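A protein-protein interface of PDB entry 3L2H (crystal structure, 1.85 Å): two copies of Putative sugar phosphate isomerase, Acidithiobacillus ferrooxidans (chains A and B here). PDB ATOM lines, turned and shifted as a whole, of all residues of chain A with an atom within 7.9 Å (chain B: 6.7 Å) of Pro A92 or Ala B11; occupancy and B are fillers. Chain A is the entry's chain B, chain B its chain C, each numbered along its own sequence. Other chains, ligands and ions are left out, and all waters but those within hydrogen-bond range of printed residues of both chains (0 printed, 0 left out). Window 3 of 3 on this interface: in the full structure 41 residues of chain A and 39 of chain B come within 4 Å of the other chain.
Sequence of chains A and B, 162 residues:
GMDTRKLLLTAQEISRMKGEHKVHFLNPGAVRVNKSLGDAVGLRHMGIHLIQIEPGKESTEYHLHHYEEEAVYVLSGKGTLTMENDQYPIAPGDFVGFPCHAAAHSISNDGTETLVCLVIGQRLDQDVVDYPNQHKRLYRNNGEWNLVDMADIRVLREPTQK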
ATOM      1  N   TYR A  73     -14.991  -1.539  -5.184  1.00  0.00           N
ATOM      2  CA  TYR A  73     -14.210  -1.012  -6.316  1.00  0.00           C
ATOM      3  C   TYR A  73     -14.717   0.390  -6.614  1.00  0.00           C
ATOM      4  O   TYR A  73     -15.915   0.600  -6.821  1.00  0.00           O
ATOM      5  CB  TYR A  73     -14.260  -1.932  -7.553  1.00  0.00           C
ATOM      6  CG  TYR A  73     -13.372  -1.480  -8.712  1.00  0.00           C
ATOM      7  CD1 TYR A  73     -12.050  -1.869  -8.768  1.00  0.00           C
ATOM      8  CD2 TYR A  73     -13.849  -0.675  -9.734  1.00  0.00           C
ATOM      9  CE1 TYR A  73     -11.207  -1.475  -9.803  1.00  0.00           C
ATOM     10  CE2 TYR A  73     -12.994  -0.260 -10.782  1.00  0.00           C
ATOM     11  CZ  TYR A  73     -11.675  -0.671 -10.804  1.00  0.00           C
ATOM     12  OH  TYR A  73     -10.799  -0.340 -11.820  1.00  0.00           O
ATOM     13  N   VAL A  74     -13.829   1.365  -6.545  1.00  0.00           N
ATOM     14  CA  VAL A  74     -14.243   2.771  -6.666  1.00  0.00           C
ATOM     15  C   VAL A  74     -14.336   3.156  -8.125  1.00  0.00           C
ATOM     16  O   VAL A  74     -13.363   3.038  -8.856  1.00  0.00           O
ATOM     17  CB  VAL A  74     -13.284   3.715  -5.958  1.00  0.00           C
ATOM     18  CG1 VAL A  74     -13.779   5.193  -6.071  1.00  0.00           C
ATOM     19  CG2 VAL A  74     -13.098   3.323  -4.485  1.00  0.00           C
ATOM     20  N   LEU A  75     -15.510   3.618  -8.542  1.00  0.00           N
ATOM     21  CA  LEU A  75     -15.735   4.057  -9.914  1.00  0.00           C
ATOM     22  C   LEU A  75     -15.520   5.556 -10.079  1.00  0.00           C
ATOM     23  O   LEU A  75     -14.971   5.970 -11.089  1.00  0.00           O
ATOM     24  CB  LEU A  75     -17.143   3.679 -10.376  1.00  0.00           C
ATOM     25  CG  LEU A  75     -17.415   2.169 -10.448  1.00  0.00           C
ATOM     26  CD1 LEU A  75     -18.927   1.868 -10.751  1.00  0.00           C
ATOM     27  CD2 LEU A  75     -16.503   1.457 -11.450  1.00  0.00           C
ATOM     28  N   SER A  76     -15.996   6.373  -9.138  1.00  0.00           N
ATOM     29  CA  SER A  76     -15.740   7.817  -9.233  1.00  0.00           C
ATOM     30  C   SER A  76     -15.849   8.474  -7.888  1.00  0.00           C
ATOM     31  O   SER A  76     -16.430   7.917  -6.935  1.00  0.00           O
ATOM     32  CB  SER A  76     -16.685   8.528 -10.211  1.00  0.00           C
ATOM     33  OG  SER A  76     -18.002   8.532  -9.758  1.00  0.00           O
ATOM     34  N   GLY A  77     -15.279   9.673  -7.830  1.00  0.00           N
ATOM     35  CA  GLY A  77     -15.182  10.444  -6.616  1.00  0.00           C
ATOM     36  C   GLY A  77     -14.129   9.910  -5.654  1.00  0.00           C
ATOM     37  O   GLY A  77     -13.362   9.003  -5.999  1.00  0.00           O
ATOM     38  N   LYS A  78     -14.140  10.456  -4.436  1.00  0.00           N
ATOM     39  CA  LYS A  78     -13.140  10.165  -3.417  1.00  0.00           C
ATOM     40  C   LYS A  78     -13.762   9.885  -2.077  1.00  0.00           C
ATOM     41  O   LYS A  78     -14.839  10.353  -1.788  1.00  0.00           O
ATOM     42  CB  LYS A  78     -12.203  11.362  -3.282  1.00  0.00           C
ATOM     43  CG  LYS A  78     -11.452  11.692  -4.557  1.00  0.00           C
ATOM     44  CD  LYS A  78     -10.595  12.933  -4.421  1.00  0.00           C
ATOM     45  CE  LYS A  78      -9.535  13.028  -5.562  1.00  0.00           C
ATOM     46  NZ  LYS A  78      -8.844  14.395  -5.597  1.00  0.00           N
ATOM     47  N   GLY A  79     -13.063   9.110  -1.250  1.00  0.00           N
ATOM     48  CA  GLY A  79     -13.560   8.764   0.071  1.00  0.00           C
ATOM     49  C   GLY A  79     -12.435   8.553   1.046  1.00  0.00           C
ATOM     50  O   GLY A  79     -11.267   8.648   0.688  1.00  0.00           O
ATOM     51  N   ILE A  90      -9.212   6.973  -0.578  1.00  0.00           N
ATOM     52  CA  ILE A  90      -9.489   6.136  -1.725  1.00  0.00           C
ATOM     53  C   ILE A  90     -10.029   7.012  -2.851  1.00  0.00           C
ATOM     54  O   ILE A  90     -10.563   8.109  -2.619  1.00  0.00           O
ATOM     55  CB  ILE A  90     -10.442   4.968  -1.396  1.00  0.00           C
ATOM     56  CG1 ILE A  90     -11.784   5.465  -0.824  1.00  0.00           C
ATOM     57  CG2 ILE A  90      -9.760   3.992  -0.432  1.00  0.00           C
ATOM     58  CD1 ILE A  90     -12.849   4.322  -0.708  1.00  0.00           C
ATOM     59  N   ALA A  91      -9.842   6.533  -4.072  1.00  0.00           N
ATOM     60  CA  ALA A  91     -10.117   7.283  -5.257  1.00  0.00           C
ATOM     61  C   ALA A  91     -10.399   6.316  -6.396  1.00  0.00           C
ATOM     62  O   ALA A  91     -10.172   5.113  -6.256  1.00  0.00           O
ATOM     63  CB  ALA A  91      -8.893   8.211  -5.584  1.00  0.00           C
ATOM     64  N   PRO A  92     -10.849   6.830  -7.540  1.00  0.00           N
ATOM     65  CA  PRO A  92     -11.263   5.967  -8.670  1.00  0.00           C
ATOM     66  C   PRO A  92     -10.199   4.948  -9.136  1.00  0.00           C
ATOM     67  O   PRO A  92      -9.009   5.231  -9.265  1.00  0.00           O
ATOM     68  CB  PRO A  92     -11.611   6.952  -9.791  1.00  0.00           C
ATOM     69  CG  PRO A  92     -11.829   8.278  -9.099  1.00  0.00           C
ATOM     70  CD  PRO A  92     -10.883   8.266  -7.907  1.00  0.00           C
ATOM     71  N   GLY A  93     -10.666   3.716  -9.279  1.00  0.00           N
ATOM     72  CA  GLY A  93      -9.798   2.600  -9.657  1.00  0.00           C
ATOM     73  C   GLY A  93      -9.209   1.845  -8.496  1.00  0.00           C
ATOM     74  O   GLY A  93      -8.534   0.816  -8.688  1.00  0.00           O
ATOM     75  N   ASP A  94      -9.388   2.347  -7.286  1.00  0.00           N
ATOM     76  CA  ASP A  94      -8.908   1.623  -6.092  1.00  0.00           C
ATOM     77  C   ASP A  94      -9.818   0.426  -5.768  1.00  0.00           C
ATOM     78  O   ASP A  94     -11.008   0.435  -6.016  1.00  0.00           O
ATOM     79  CB  ASP A  94      -8.861   2.499  -4.850  1.00  0.00           C
ATOM     80  CG  ASP A  94      -7.824   3.625  -4.913  1.00  0.00           C
ATOM     81  OD1 ASP A  94      -6.988   3.714  -5.882  1.00  0.00           O
ATOM     82  OD2 ASP A  94      -7.900   4.456  -3.951  1.00  0.00           O
ATOM     83  N   PHE A  95      -9.239  -0.585  -5.139  1.00  0.00           N
ATOM     84  CA  PHE A  95      -9.938  -1.768  -4.772  1.00  0.00           C
ATOM     85  C   PHE A  95      -9.567  -2.130  -3.364  1.00  0.00           C
ATOM     86  O   PHE A  95      -8.369  -2.131  -3.016  1.00  0.00           O
ATOM     87  CB  PHE A  95      -9.505  -2.899  -5.695  1.00  0.00           C
ATOM     88  CG  PHE A  95     -10.087  -4.261  -5.327  1.00  0.00           C
ATOM     89  CD1 PHE A  95     -11.357  -4.621  -5.715  1.00  0.00           C
ATOM     90  CD2 PHE A  95      -9.355  -5.155  -4.548  1.00  0.00           C
ATOM     91  CE1 PHE A  95     -11.879  -5.882  -5.352  1.00  0.00           C
ATOM     92  CE2 PHE A  95      -9.857  -6.389  -4.218  1.00  0.00           C
ATOM     93  CZ  PHE A  95     -11.125  -6.748  -4.620  1.00  0.00           C
ATOM     94  N   GLU A 113     -17.733  15.591  -4.380  1.00  0.00           N
ATOM     95  CA  GLU A 113     -18.570  14.986  -5.413  1.00  0.00           C
ATOM     96  C   GLU A 113     -19.082  13.656  -4.878  1.00  0.00           C
ATOM     97  O   GLU A 113     -18.586  13.142  -3.882  1.00  0.00           O
ATOM     98  CB  GLU A 113     -17.812  14.817  -6.739  1.00  0.00           C
ATOM     99  CG  GLU A 113     -16.782  13.715  -6.757  1.00  0.00           C
ATOM    100  CD  GLU A 113     -15.932  13.694  -8.032  1.00  0.00           C
ATOM    101  OE1 GLU A 113     -16.343  13.096  -9.075  1.00  0.00           O
ATOM    102  OE2 GLU A 113     -14.802  14.222  -7.939  1.00  0.00           O
ATOM    103  N   LEU A 115     -19.568   9.858  -4.215  1.00  0.00           N
ATOM    104  CA  LEU A 115     -18.664   8.701  -4.233  1.00  0.00           C
ATOM    105  C   LEU A 115     -19.438   7.558  -4.820  1.00  0.00           C
ATOM    106  O   LEU A 115     -20.490   7.196  -4.272  1.00  0.00           O
ATOM    107  CB  LEU A 115     -18.155   8.403  -2.837  1.00  0.00           C
ATOM    108  CG  LEU A 115     -17.335   7.130  -2.615  1.00  0.00           C
ATOM    109  CD1 LEU A 115     -16.076   7.093  -3.499  1.00  0.00           C
ATOM    110  CD2 LEU A 115     -16.928   7.007  -1.134  1.00  0.00           C
ATOM    111  N   VAL A 116     -18.950   6.988  -5.933  1.00  0.00           N
ATOM    112  CA  VAL A 116     -19.666   5.923  -6.623  1.00  0.00           C
ATOM    113  C   VAL A 116     -18.789   4.659  -6.699  1.00  0.00           C
ATOM    114  O   VAL A 116     -17.668   4.694  -7.176  1.00  0.00           O
ATOM    115  CB  VAL A 116     -20.144   6.369  -8.033  1.00  0.00           C
ATOM    116  CG1 VAL A 116     -20.952   5.269  -8.747  1.00  0.00           C
ATOM    117  CG2 VAL A 116     -20.953   7.687  -7.912  1.00  0.00           C
ATOM    118  N   LEU B   9      -5.655  -2.068  -2.646  1.00  0.00           N
ATOM    119  CA  LEU B   9      -4.851  -1.912  -3.851  1.00  0.00           C
ATOM    120  C   LEU B   9      -5.224  -0.596  -4.503  1.00  0.00           C
ATOM    121  O   LEU B   9      -6.374  -0.433  -4.937  1.00  0.00           O
ATOM    122  CB  LEU B   9      -5.121  -3.035  -4.843  1.00  0.00           C
ATOM    123  CG  LEU B   9      -4.943  -4.451  -4.364  1.00  0.00           C
ATOM    124  CD1 LEU B   9      -5.504  -5.421  -5.436  1.00  0.00           C
ATOM    125  CD2 LEU B   9      -3.462  -4.767  -4.043  1.00  0.00           C
ATOM    126  N   THR B  10      -4.290   0.354  -4.568  1.00  0.00           N
ATOM    127  CA  THR B  10      -4.571   1.612  -5.266  1.00  0.00           C
ATOM    128  C   THR B  10      -4.661   1.382  -6.792  1.00  0.00           C
ATOM    129  O   THR B  10      -4.164   0.385  -7.335  1.00  0.00           O
ATOM    130  CB  THR B  10      -3.490   2.686  -4.994  1.00  0.00           C
ATOM    131  OG1 THR B  10      -2.245   2.235  -5.537  1.00  0.00           O
ATOM    132  CG2 THR B  10      -3.309   2.963  -3.503  1.00  0.00           C
ATOM    133  N   ALA B  11      -5.290   2.311  -7.491  1.00  0.00           N
ATOM    134  CA  ALA B  11      -5.381   2.242  -8.931  1.00  0.00           C
ATOM    135  C   ALA B  11      -3.976   2.096  -9.524  1.00  0.00           C
ATOM    136  O   ALA B  11      -3.757   1.359 -10.479  1.00  0.00           O
ATOM    137  CB  ALA B  11      -6.057   3.490  -9.472  1.00  0.00           C
ATOM    138  N   GLN B  12      -3.018   2.822  -8.951  1.00  0.00           N
ATOM    139  CA  GLN B  12      -1.640   2.735  -9.424  1.00  0.00           C
ATOM    140  C   GLN B  12      -1.045   1.337  -9.212  1.00  0.00           C
ATOM    141  O   GLN B  12      -0.360   0.811 -10.088  1.00  0.00           O
ATOM    142  CB  GLN B  12      -0.755   3.775  -8.735  1.00  0.00           C
ATOM    143  CG  GLN B  12       0.643   3.780  -9.319  1.00  0.00           C
ATOM    144  CD  GLN B  12       1.535   4.884  -8.790  1.00  0.00           C
ATOM    145  OE1 GLN B  12       2.138   4.773  -7.712  1.00  0.00           O
ATOM    146  NE2 GLN B  12       1.664   5.945  -9.576  1.00  0.00           N
ATOM    147  N   GLU B  13      -1.283   0.752  -8.041  1.00  0.00           N
ATOM    148  CA  GLU B  13      -0.778  -0.592  -7.767  1.00  0.00           C
ATOM    149  C   GLU B  13      -1.336  -1.578  -8.796  1.00  0.00           C
ATOM    150  O   GLU B  13      -0.604  -2.467  -9.287  1.00  0.00           O
ATOM    151  CB  GLU B  13      -1.123  -1.044  -6.358  1.00  0.00           C
ATOM    152  CG  GLU B  13      -0.307  -0.464  -5.188  1.00  0.00           C
ATOM    153  CD  GLU B  13      -0.955  -0.847  -3.839  1.00  0.00           C
ATOM    154  OE1 GLU B  13      -0.681  -1.937  -3.305  1.00  0.00           O
ATOM    155  OE2 GLU B  13      -1.832  -0.121  -3.341  1.00  0.00           O
ATOM    156  N   ILE B  14      -2.616  -1.410  -9.123  1.00  0.00           N
ATOM    157  CA  ILE B  14      -3.295  -2.294 -10.069  1.00  0.00           C
ATOM    158  C   ILE B  14      -2.686  -2.123 -11.451  1.00  0.00           C
ATOM    159  O   ILE B  14      -2.434  -3.139 -12.130  1.00  0.00           O
ATOM    160  CB  ILE B  14      -4.811  -2.083 -10.068  1.00  0.00           C
ATOM    161  CG1 ILE B  14      -5.356  -2.563  -8.720  1.00  0.00           C
ATOM    162  CG2 ILE B  14      -5.494  -2.857 -11.193  1.00  0.00           C
ATOM    163  CD1 ILE B  14      -6.835  -2.343  -8.471  1.00  0.00           C
ATOM    164  N   SER B  15      -2.507  -0.861 -11.883  1.00  0.00           N
ATOM    165  CA  SER B  15      -1.862  -0.559 -13.158  1.00  0.00           C
ATOM    166  C   SER B  15      -0.556  -1.294 -13.307  1.00  0.00           C
ATOM    167  O   SER B  15      -0.258  -1.824 -14.363  1.00  0.00           O
ATOM    168  CB  SER B  15      -1.523   0.929 -13.306  1.00  0.00           C
ATOM    169  OG  SER B  15      -2.606   1.643 -13.830  1.00  0.00           O
ATOM    170  N   ARG B  16       0.234  -1.259 -12.228  1.00  0.00           N
ATOM    171  CA  ARG B  16       1.582  -1.853 -12.147  1.00  0.00           C
ATOM    172  C   ARG B  16       1.630  -3.371 -12.077  1.00  0.00           C
ATOM    173  O   ARG B  16       2.601  -3.985 -12.519  1.00  0.00           O
ATOM    174  CB  ARG B  16       2.316  -1.353 -10.896  1.00  0.00           C
ATOM    175  CG  ARG B  16       2.836   0.057 -10.984  1.00  0.00           C
ATOM    176  CD  ARG B  16       3.706   0.466  -9.781  1.00  0.00           C
ATOM    177  NE  ARG B  16       4.237   1.807 -10.024  1.00  0.00           N
ATOM    178  CZ  ARG B  16       4.941   2.548  -9.173  1.00  0.00           C
ATOM    179  NH1 ARG B  16       5.240   2.119  -7.956  1.00  0.00           N
ATOM    180  NH2 ARG B  16       5.335   3.750  -9.566  1.00  0.00           N
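Among the printed residues, pairs that only touch across the chains: Asp A94 with Thr B10 (3.3 Å), Pro A92 with Ala B11 (3.4 Å), Asp A94 with Leu B9 (3.5 Å), Gly A93 with Ala B11 (3.5 Å), Gly A93 with Ile B14 (3.6 Å) and Phe A95 with Ile B14 (3.9 Å).
No position is printed for both chains. Of the 8 pairs that touch across the chains among the printed residues, none has its exchanged pair printed and touching as well.
Pro A92 touches one residue of chain B. Of chain A, only Pro A92, Gly A93 and Asp A94 come within 4 Å of Ala B11. Of the printed residues of chain B, Gly A93 touches Ala B11 (3.5 Å) and Ile B14 (3.6 Å). Of the printed residues of chain A, Ile B14 touches Gly A93 (3.6 Å) and Phe A95 (3.9 Å). Printed residues of chain B within 4 Å of Phe A95: Leu B9 and Ile B14. Ser A76 touches none of the printed residues of chain B. The nearest printed residue of chain B that does not touch Phe A95 is Thr B10 (5.0 Å).
Hydrophobic or aromatic side chains of chain B that line the printed part of chain A: Leu B9, Ala B11 and Ile B14. Along chain B the printed residues that touch a printed residue of chain A span positions 9 to 14.
N of Thr B10 sits at hydrogen-bond distance from OE2 of Glu B13. The backbone carbonyl oxygen (O) of Val A74 lies within hydrogen-bond range of the backbone NH (N) of Gly A93 (2.8 Å). N of Val A74 is in hydrogen-bond range of O of Asp A94, at 3.0 Å. The side-chain carboxylate (OD2) of Asp A94 sits at hydrogen-bond distance from the backbone NH (N) of Ala A91 (2.8 Å).
N of Leu B9 sits at hydrogen-bond distance from O of Phe A95 (2.7 Å). N of Ala B11 is in hydrogen-bond range of OD1 of Asp A94 (2.7 Å).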
